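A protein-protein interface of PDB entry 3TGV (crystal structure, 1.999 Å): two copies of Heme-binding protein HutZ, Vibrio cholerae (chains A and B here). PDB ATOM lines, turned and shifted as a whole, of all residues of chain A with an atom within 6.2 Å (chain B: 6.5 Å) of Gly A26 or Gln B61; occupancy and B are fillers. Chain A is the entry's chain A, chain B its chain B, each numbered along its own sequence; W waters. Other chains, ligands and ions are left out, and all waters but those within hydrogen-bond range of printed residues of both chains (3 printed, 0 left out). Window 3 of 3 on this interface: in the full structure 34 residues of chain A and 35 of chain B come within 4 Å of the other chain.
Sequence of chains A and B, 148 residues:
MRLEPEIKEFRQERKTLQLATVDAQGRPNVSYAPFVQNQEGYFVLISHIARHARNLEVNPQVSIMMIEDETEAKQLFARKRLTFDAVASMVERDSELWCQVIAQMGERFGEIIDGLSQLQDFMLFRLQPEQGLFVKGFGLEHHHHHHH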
ATOM      1  N   VAL A  22      20.333  16.805 -26.325  1.00  0.00           N
ATOM      2  CA  VAL A  22      21.391  15.819 -26.115  1.00  0.00           C
ATOM      3  C   VAL A  22      22.106  15.530 -27.422  1.00  0.00           C
ATOM      4  O   VAL A  22      21.480  15.513 -28.484  1.00  0.00           O
ATOM      5  CB  VAL A  22      20.846  14.498 -25.546  1.00  0.00           C
ATOM      6  CG1 VAL A  22      20.665  14.592 -24.042  1.00  0.00           C
ATOM      7  CG2 VAL A  22      19.533  14.132 -26.235  1.00  0.00           C
ATOM      8  N   ASP A  23      23.413  15.296 -27.350  1.00  0.00           N
ATOM      9  CA  ASP A  23      24.141  14.895 -28.544  1.00  0.00           C
ATOM     10  C   ASP A  23      24.019  13.380 -28.748  1.00  0.00           C
ATOM     11  O   ASP A  23      23.348  12.704 -27.980  1.00  0.00           O
ATOM     12  CB  ASP A  23      25.602  15.357 -28.494  1.00  0.00           C
ATOM     13  CG  ASP A  23      26.420  14.615 -27.462  1.00  0.00           C
ATOM     14  OD1 ASP A  23      27.558  15.062 -27.173  1.00  0.00           O
ATOM     15  OD2 ASP A  23      25.927  13.580 -26.957  1.00  0.00           O
ATOM     16  N   ALA A  24      24.659  12.852 -29.783  1.00  0.00           N
ATOM     17  CA  ALA A  24      24.478  11.447 -30.156  1.00  0.00           C
ATOM     18  C   ALA A  24      24.848  10.468 -29.043  1.00  0.00           C
ATOM     19  O   ALA A  24      24.330   9.350 -28.990  1.00  0.00           O
ATOM     20  CB  ALA A  24      25.262  11.132 -31.426  1.00  0.00           C
ATOM     21  N   GLN A  25      25.742  10.891 -28.155  1.00  0.00           N
ATOM     22  CA  GLN A  25      26.134  10.068 -27.017  1.00  0.00           C
ATOM     23  C   GLN A  25      25.361  10.433 -25.754  1.00  0.00           C
ATOM     24  O   GLN A  25      25.661   9.941 -24.670  1.00  0.00           O
ATOM     25  CB  GLN A  25      27.633  10.190 -26.755  1.00  0.00           C
ATOM     26  CG  GLN A  25      28.515   9.559 -27.835  1.00  0.00           C
ATOM     27  CD  GLN A  25      28.426  10.274 -29.170  1.00  0.00           C
ATOM     28  OE1 GLN A  25      28.764  11.459 -29.287  1.00  0.00           O
ATOM     29  NE2 GLN A  25      27.972   9.551 -30.194  1.00  0.00           N
ATOM     30  N   GLY A  26      24.365  11.300 -25.893  1.00  0.00           N
ATOM     31  CA  GLY A  26      23.548  11.689 -24.754  1.00  0.00           C
ATOM     32  C   GLY A  26      24.197  12.618 -23.738  1.00  0.00           C
ATOM     33  O   GLY A  26      23.831  12.599 -22.569  1.00  0.00           O
ATOM     34  N   ARG A  27      25.156  13.435 -24.171  1.00  0.00           N
ATOM     35  CA  ARG A  27      25.636  14.532 -23.337  1.00  0.00           C
ATOM     36  C   ARG A  27      24.607  15.664 -23.385  1.00  0.00           C
ATOM     37  O   ARG A  27      24.242  16.117 -24.477  1.00  0.00           O
ATOM     38  CB  ARG A  27      26.996  15.051 -23.844  1.00  0.00           C
ATOM     39  CG  ARG A  27      28.090  14.001 -23.876  1.00  0.00           C
ATOM     40  CD  ARG A  27      29.347  14.529 -24.546  1.00  0.00           C
ATOM     41  NE  ARG A  27      30.305  13.461 -24.805  1.00  0.00           N
ATOM     42  CZ  ARG A  27      30.395  12.803 -25.955  1.00  0.00           C
ATOM     43  NH1 ARG A  27      29.579  13.103 -26.960  1.00  0.00           N
ATOM     44  NH2 ARG A  27      31.308  11.847 -26.104  1.00  0.00           N
ATOM     45  N   PRO A  28      24.138  16.126 -22.208  1.00  0.00           N
ATOM     46  CA  PRO A  28      23.099  17.162 -22.095  1.00  0.00           C
ATOM     47  C   PRO A  28      23.587  18.566 -22.467  1.00  0.00           C
ATOM     48  O   PRO A  28      24.736  18.924 -22.240  1.00  0.00           O
ATOM     49  CB  PRO A  28      22.781  17.169 -20.600  1.00  0.00           C
ATOM     50  CG  PRO A  28      24.082  16.766 -19.968  1.00  0.00           C
ATOM     51  CD  PRO A  28      24.639  15.712 -20.887  1.00  0.00           C
ATOM     52  N   ASN A  59      19.872  13.875 -32.594  1.00  0.00           N
ATOM     53  CA  ASN A  59      19.173  13.202 -31.517  1.00  0.00           C
ATOM     54  C   ASN A  59      17.924  14.012 -31.177  1.00  0.00           C
ATOM     55  O   ASN A  59      17.971  14.923 -30.353  1.00  0.00           O
ATOM     56  CB  ASN A  59      20.097  13.088 -30.305  1.00  0.00           C
ATOM     57  CG  ASN A  59      19.526  12.202 -29.223  1.00  0.00           C
ATOM     58  OD1 ASN A  59      18.309  12.064 -29.108  1.00  0.00           O
ATOM     59  ND2 ASN A  59      20.401  11.595 -28.420  1.00  0.00           N
ATOM     60  N   ALA B  20      20.131  21.159 -17.590  1.00  0.00           N
ATOM     61  CA  ALA B  20      19.803  20.085 -18.503  1.00  0.00           C
ATOM     62  C   ALA B  20      20.463  18.840 -17.961  1.00  0.00           C
ATOM     63  O   ALA B  20      21.694  18.783 -17.851  1.00  0.00           O
ATOM     64  CB  ALA B  20      20.297  20.392 -19.915  1.00  0.00           C
ATOM     65  N   THR B  21      19.629  17.868 -17.594  1.00  0.00           N
ATOM     66  CA  THR B  21      20.070  16.590 -17.042  1.00  0.00           C
ATOM     67  C   THR B  21      19.617  15.447 -17.961  1.00  0.00           C
ATOM     68  O   THR B  21      18.886  15.677 -18.937  1.00  0.00           O
ATOM     69  CB  THR B  21      19.557  16.387 -15.588  1.00  0.00           C
ATOM     70  OG1 THR B  21      18.122  16.367 -15.569  1.00  0.00           O
ATOM     71  CG2 THR B  21      20.030  17.544 -14.710  1.00  0.00           C
ATOM     72  N   VAL B  22      20.074  14.230 -17.676  1.00  0.00           N
ATOM     73  CA  VAL B  22      19.739  13.059 -18.487  1.00  0.00           C
ATOM     74  C   VAL B  22      19.499  11.858 -17.596  1.00  0.00           C
ATOM     75  O   VAL B  22      20.182  11.689 -16.582  1.00  0.00           O
ATOM     76  CB  VAL B  22      20.881  12.701 -19.479  1.00  0.00           C
ATOM     77  CG1 VAL B  22      20.727  13.474 -20.775  1.00  0.00           C
ATOM     78  CG2 VAL B  22      22.262  12.952 -18.844  1.00  0.00           C
ATOM     79  N   GLN B  25      19.069   6.277 -19.738  1.00  0.00           N
ATOM     80  CA  GLN B  25      19.121   6.035 -21.177  1.00  0.00           C
ATOM     81  C   GLN B  25      19.415   7.308 -21.976  1.00  0.00           C
ATOM     82  O   GLN B  25      19.253   7.326 -23.192  1.00  0.00           O
ATOM     83  CB  GLN B  25      17.831   5.400 -21.685  1.00  0.00           C
ATOM     84  CG  GLN B  25      16.728   5.296 -20.658  1.00  0.00           C
ATOM     85  CD  GLN B  25      16.613   3.912 -20.041  1.00  0.00           C
ATOM     86  OE1 GLN B  25      17.451   3.508 -19.226  1.00  0.00           O
ATOM     87  NE2 GLN B  25      15.564   3.177 -20.423  1.00  0.00           N
ATOM     88  N   GLY B  26      19.833   8.370 -21.292  1.00  0.00           N
ATOM     89  CA  GLY B  26      20.228   9.597 -21.965  1.00  0.00           C
ATOM     90  C   GLY B  26      19.086  10.440 -22.501  1.00  0.00           C
ATOM     91  O   GLY B  26      19.245  11.148 -23.490  1.00  0.00           O
ATOM     92  N   ARG B  27      17.926  10.370 -21.855  1.00  0.00           N
ATOM     93  CA  ARG B  27      16.810  11.230 -22.235  1.00  0.00           C
ATOM     94  C   ARG B  27      16.879  12.516 -21.443  1.00  0.00           C
ATOM     95  O   ARG B  27      16.997  12.476 -20.222  1.00  0.00           O
ATOM     96  CB  ARG B  27      15.486  10.555 -21.936  1.00  0.00           C
ATOM     97  CG  ARG B  27      15.369   9.161 -22.451  1.00  0.00           C
ATOM     98  CD  ARG B  27      14.561   8.358 -21.444  1.00  0.00           C
ATOM     99  NE  ARG B  27      13.821   7.296 -22.088  1.00  0.00           N
ATOM    100  CZ  ARG B  27      13.527   6.142 -21.507  1.00  0.00           C
ATOM    101  NH1 ARG B  27      13.925   5.897 -20.264  1.00  0.00           N
ATOM    102  NH2 ARG B  27      12.852   5.233 -22.188  1.00  0.00           N
ATOM    103  N   ASN B  55      17.884  12.015 -12.144  1.00  0.00           N
ATOM    104  CA  ASN B  55      18.840  12.041 -13.251  1.00  0.00           C
ATOM    105  C   ASN B  55      20.271  12.287 -12.769  1.00  0.00           C
ATOM    106  O   ASN B  55      21.178  11.563 -13.134  1.00  0.00           O
ATOM    107  CB  ASN B  55      18.460  13.100 -14.303  1.00  0.00           C
ATOM    108  CG  ASN B  55      17.286  12.673 -15.161  1.00  0.00           C
ATOM    109  OD1 ASN B  55      16.849  11.517 -15.107  1.00  0.00           O
ATOM    110  ND2 ASN B  55      16.773  13.597 -15.969  1.00  0.00           N
ATOM    111  N   LEU B  56      20.467  13.303 -11.936  1.00  0.00           N
ATOM    112  CA  LEU B  56      21.806  13.627 -11.447  1.00  0.00           C
ATOM    113  C   LEU B  56      22.419  12.495 -10.648  1.00  0.00           C
ATOM    114  O   LEU B  56      23.636  12.310 -10.634  1.00  0.00           O
ATOM    115  CB  LEU B  56      21.776  14.879 -10.591  1.00  0.00           C
ATOM    116  CG  LEU B  56      21.479  16.134 -11.396  1.00  0.00           C
ATOM    117  CD1 LEU B  56      21.515  17.356 -10.494  1.00  0.00           C
ATOM    118  CD2 LEU B  56      22.479  16.245 -12.519  1.00  0.00           C
ATOM    119  N   ASN B  59      23.065   9.600 -13.600  1.00  0.00           N
ATOM    120  CA  ASN B  59      23.847  10.038 -14.748  1.00  0.00           C
ATOM    121  C   ASN B  59      24.330  11.438 -14.444  1.00  0.00           C
ATOM    122  O   ASN B  59      23.677  12.400 -14.810  1.00  0.00           O
ATOM    123  CB  ASN B  59      22.955  10.066 -15.982  1.00  0.00           C
ATOM    124  CG  ASN B  59      23.736  10.154 -17.281  1.00  0.00           C
ATOM    125  OD1 ASN B  59      24.900  10.587 -17.318  1.00  0.00           O
ATOM    126  ND2 ASN B  59      23.087   9.756 -18.370  1.00  0.00           N
ATOM    127  N   PRO B  60      25.469  11.551 -13.742  1.00  0.00           N
ATOM    128  CA  PRO B  60      25.874  12.799 -13.088  1.00  0.00           C
ATOM    129  C   PRO B  60      26.549  13.843 -13.990  1.00  0.00           C
ATOM    130  O   PRO B  60      27.403  14.587 -13.521  1.00  0.00           O
ATOM    131  CB  PRO B  60      26.846  12.309 -12.010  1.00  0.00           C
ATOM    132  CG  PRO B  60      27.503  11.144 -12.647  1.00  0.00           C
ATOM    133  CD  PRO B  60      26.403  10.452 -13.436  1.00  0.00           C
ATOM    134  N   GLN B  61      26.173  13.907 -15.259  1.00  0.00           N
ATOM    135  CA  GLN B  61      26.586  15.033 -16.092  1.00  0.00           C
ATOM    136  C   GLN B  61      25.437  16.047 -16.185  1.00  0.00           C
ATOM    137  O   GLN B  61      24.261  15.683 -16.100  1.00  0.00           O
ATOM    138  CB  GLN B  61      27.033  14.544 -17.473  1.00  0.00           C
ATOM    139  CG  GLN B  61      26.044  13.622 -18.130  1.00  0.00           C
ATOM    140  CD  GLN B  61      26.587  12.979 -19.394  1.00  0.00           C
ATOM    141  OE1 GLN B  61      27.336  13.599 -20.159  1.00  0.00           O
ATOM    142  NE2 GLN B  61      26.196  11.731 -19.630  1.00  0.00           N
ATOM    143  N   VAL B  62      25.775  17.321 -16.322  1.00  0.00           N
ATOM    144  CA  VAL B  62      24.764  18.365 -16.365  1.00  0.00           C
ATOM    145  C   VAL B  62      25.276  19.555 -17.150  1.00  0.00           C
ATOM    146  O   VAL B  62      26.446  19.889 -17.053  1.00  0.00           O
ATOM    147  CB  VAL B  62      24.450  18.906 -14.967  1.00  0.00           C
ATOM    148  CG1 VAL B  62      23.095  19.608 -14.980  1.00  0.00           C
ATOM    149  CG2 VAL B  62      24.461  17.803 -13.969  1.00  0.00           C
ATOM    150  N   SER B  63      24.390  20.198 -17.903  1.00  0.00           N
ATOM    151  CA  SER B  63      24.707  21.456 -18.552  1.00  0.00           C
ATOM    152  C   SER B  63      23.973  22.537 -17.786  1.00  0.00           C
ATOM    153  O   SER B  63      22.775  22.422 -17.531  1.00  0.00           O
ATOM    154  CB  SER B  63      24.290  21.431 -20.023  1.00  0.00           C
ATOM    155  OG  SER B  63      24.492  22.694 -20.643  1.00  0.00           O
ATOM    156  N   ALA B  86      29.105  20.476 -16.341  1.00  0.00           N
ATOM    157  CA  ALA B  86      29.631  20.166 -15.024  1.00  0.00           C
ATOM    158  C   ALA B  86      29.405  18.705 -14.667  1.00  0.00           C
ATOM    159  O   ALA B  86      28.588  18.024 -15.281  1.00  0.00           O
ATOM    160  CB  ALA B  86      28.990  21.076 -13.973  1.00  0.00           C
ATOM    161  N   VAL B  87      30.136  18.238 -13.664  1.00  0.00           N
ATOM    162  CA  VAL B  87      29.928  16.913 -13.099  1.00  0.00           C
ATOM    163  C   VAL B  87      29.260  17.054 -11.728  1.00  0.00           C
ATOM    164  O   VAL B  87      29.661  17.891 -10.914  1.00  0.00           O
ATOM    165  CB  VAL B  87      31.257  16.175 -12.905  1.00  0.00           C
ATOM    166  CG1 VAL B  87      30.999  14.773 -12.362  1.00  0.00           C
ATOM    167  CG2 VAL B  87      32.033  16.120 -14.210  1.00  0.00           C
ATOM    168  N   ALA B  88      28.250  16.230 -11.465  1.00  0.00           N
ATOM    169  CA  ALA B  88      27.487  16.360 -10.239  1.00  0.00           C
ATOM    170  C   ALA B  88      27.817  15.239  -9.270  1.00  0.00           C
ATOM    171  O   ALA B  88      28.124  14.122  -9.678  1.00  0.00           O
ATOM    172  CB  ALA B  88      25.994  16.358 -10.544  1.00  0.00           C
HETATM  173  O   HOH W   1      20.399  10.608 -25.850  1.00  0.00           O
HETATM  174  O   HOH W   2      23.635  10.116 -21.009  1.00  0.00           O
HETATM  175  O   HOH W   3      27.147  10.744 -22.422  1.00  0.00           O
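OD2 of Asp A23 is in hydrogen-bond range of N of Gly A26, 3.0 Å away.
The side-chain carboxylate (OD1) of Asp A23 is in salt-bridge range of the guanidinium group (NH1) of Arg A27.
The side-chain amide oxygen (OE1) of Gln A25 sits at hydrogen-bond distance from the guanidinium group (NH1) of Arg A27, at 3.0 Å.
The backbone NH of Ala B20 is in hydrogen-bond range of the backbone carbonyl oxygen of Ser B63 (2.9 Å).
The side-chain amide nitrogen of Gln B61 sits at hydrogen-bond distance from the side-chain amide oxygen of Asn B59 (2.9 Å).
Val A22 touches Val B22 (CG1 to CG1, 3.5 Å).
Gly B26 touches Val A22.
Gly A26 touches Val B22.
NE2 of Gln B61 touches O of Gly A26, 3.9 Å away.
OE1 of Gln B61 touches CA of Arg A27, 3.7 Å away.
CB of Pro A28 touches O of Ala B20, at 3.4 Å.
Pro A28 touches Gln B61.
Ser B63 touches Pro A28 (CB to O, 3.4 Å).
Of the printed residues of chain B, Arg A27 touches Gln B61.
Of the printed residues of chain A, Ala B20 touches Pro A28.
Thr B21 touches none of the printed residues of chain A.
The nearest residue of chain B that does not touch Gly A26 is Gly B26 (4.5 Å).
The nearest residue of chain A that does not touch Gln B61 is Gln A25 (5.4 Å).
The nearest printed residue of chain B that does not touch Arg A27 is Val B22 (5.2 Å).
Of the 8 printed residues of chain A, 4 touch a printed residue of chain B.
Hydrophobic or aromatic side chains of chain A within 4 Å of the printed part of chain B: Val A22 and Pro A28.
Hydrophobic or aromatic side chains of chain B within 4 Å of the printed part of chain A: Val B22.
Among the printed residues, no Asp or Glu carboxylate lies within 4 Å of a Lys or Arg side-chain nitrogen of the other chain.
Val B22 touches its own counterpart, Val A22.
Val A22 touches Gly B26, and with the chains exchanged Gly A26 touches Val B22.
Water W1 lies within hydrogen-bond range of O of Gly B26 (2.7 Å) and ND2 of Asn A59 (2.8 Å).
Water W2 lies within hydrogen-bond range of the side-chain amide nitrogen (ND2) of Asn B59 (2.7 Å), the backbone carbonyl oxygen (O) of Gly A26 (2.9 Å) and the side-chain amide nitrogen (NE2) of Gln B61 (3.3 Å).
Water W3 lies within hydrogen-bond range of O of Gln A25 (2.8 Å) and NE2 of Gln B61 (3.1 Å).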
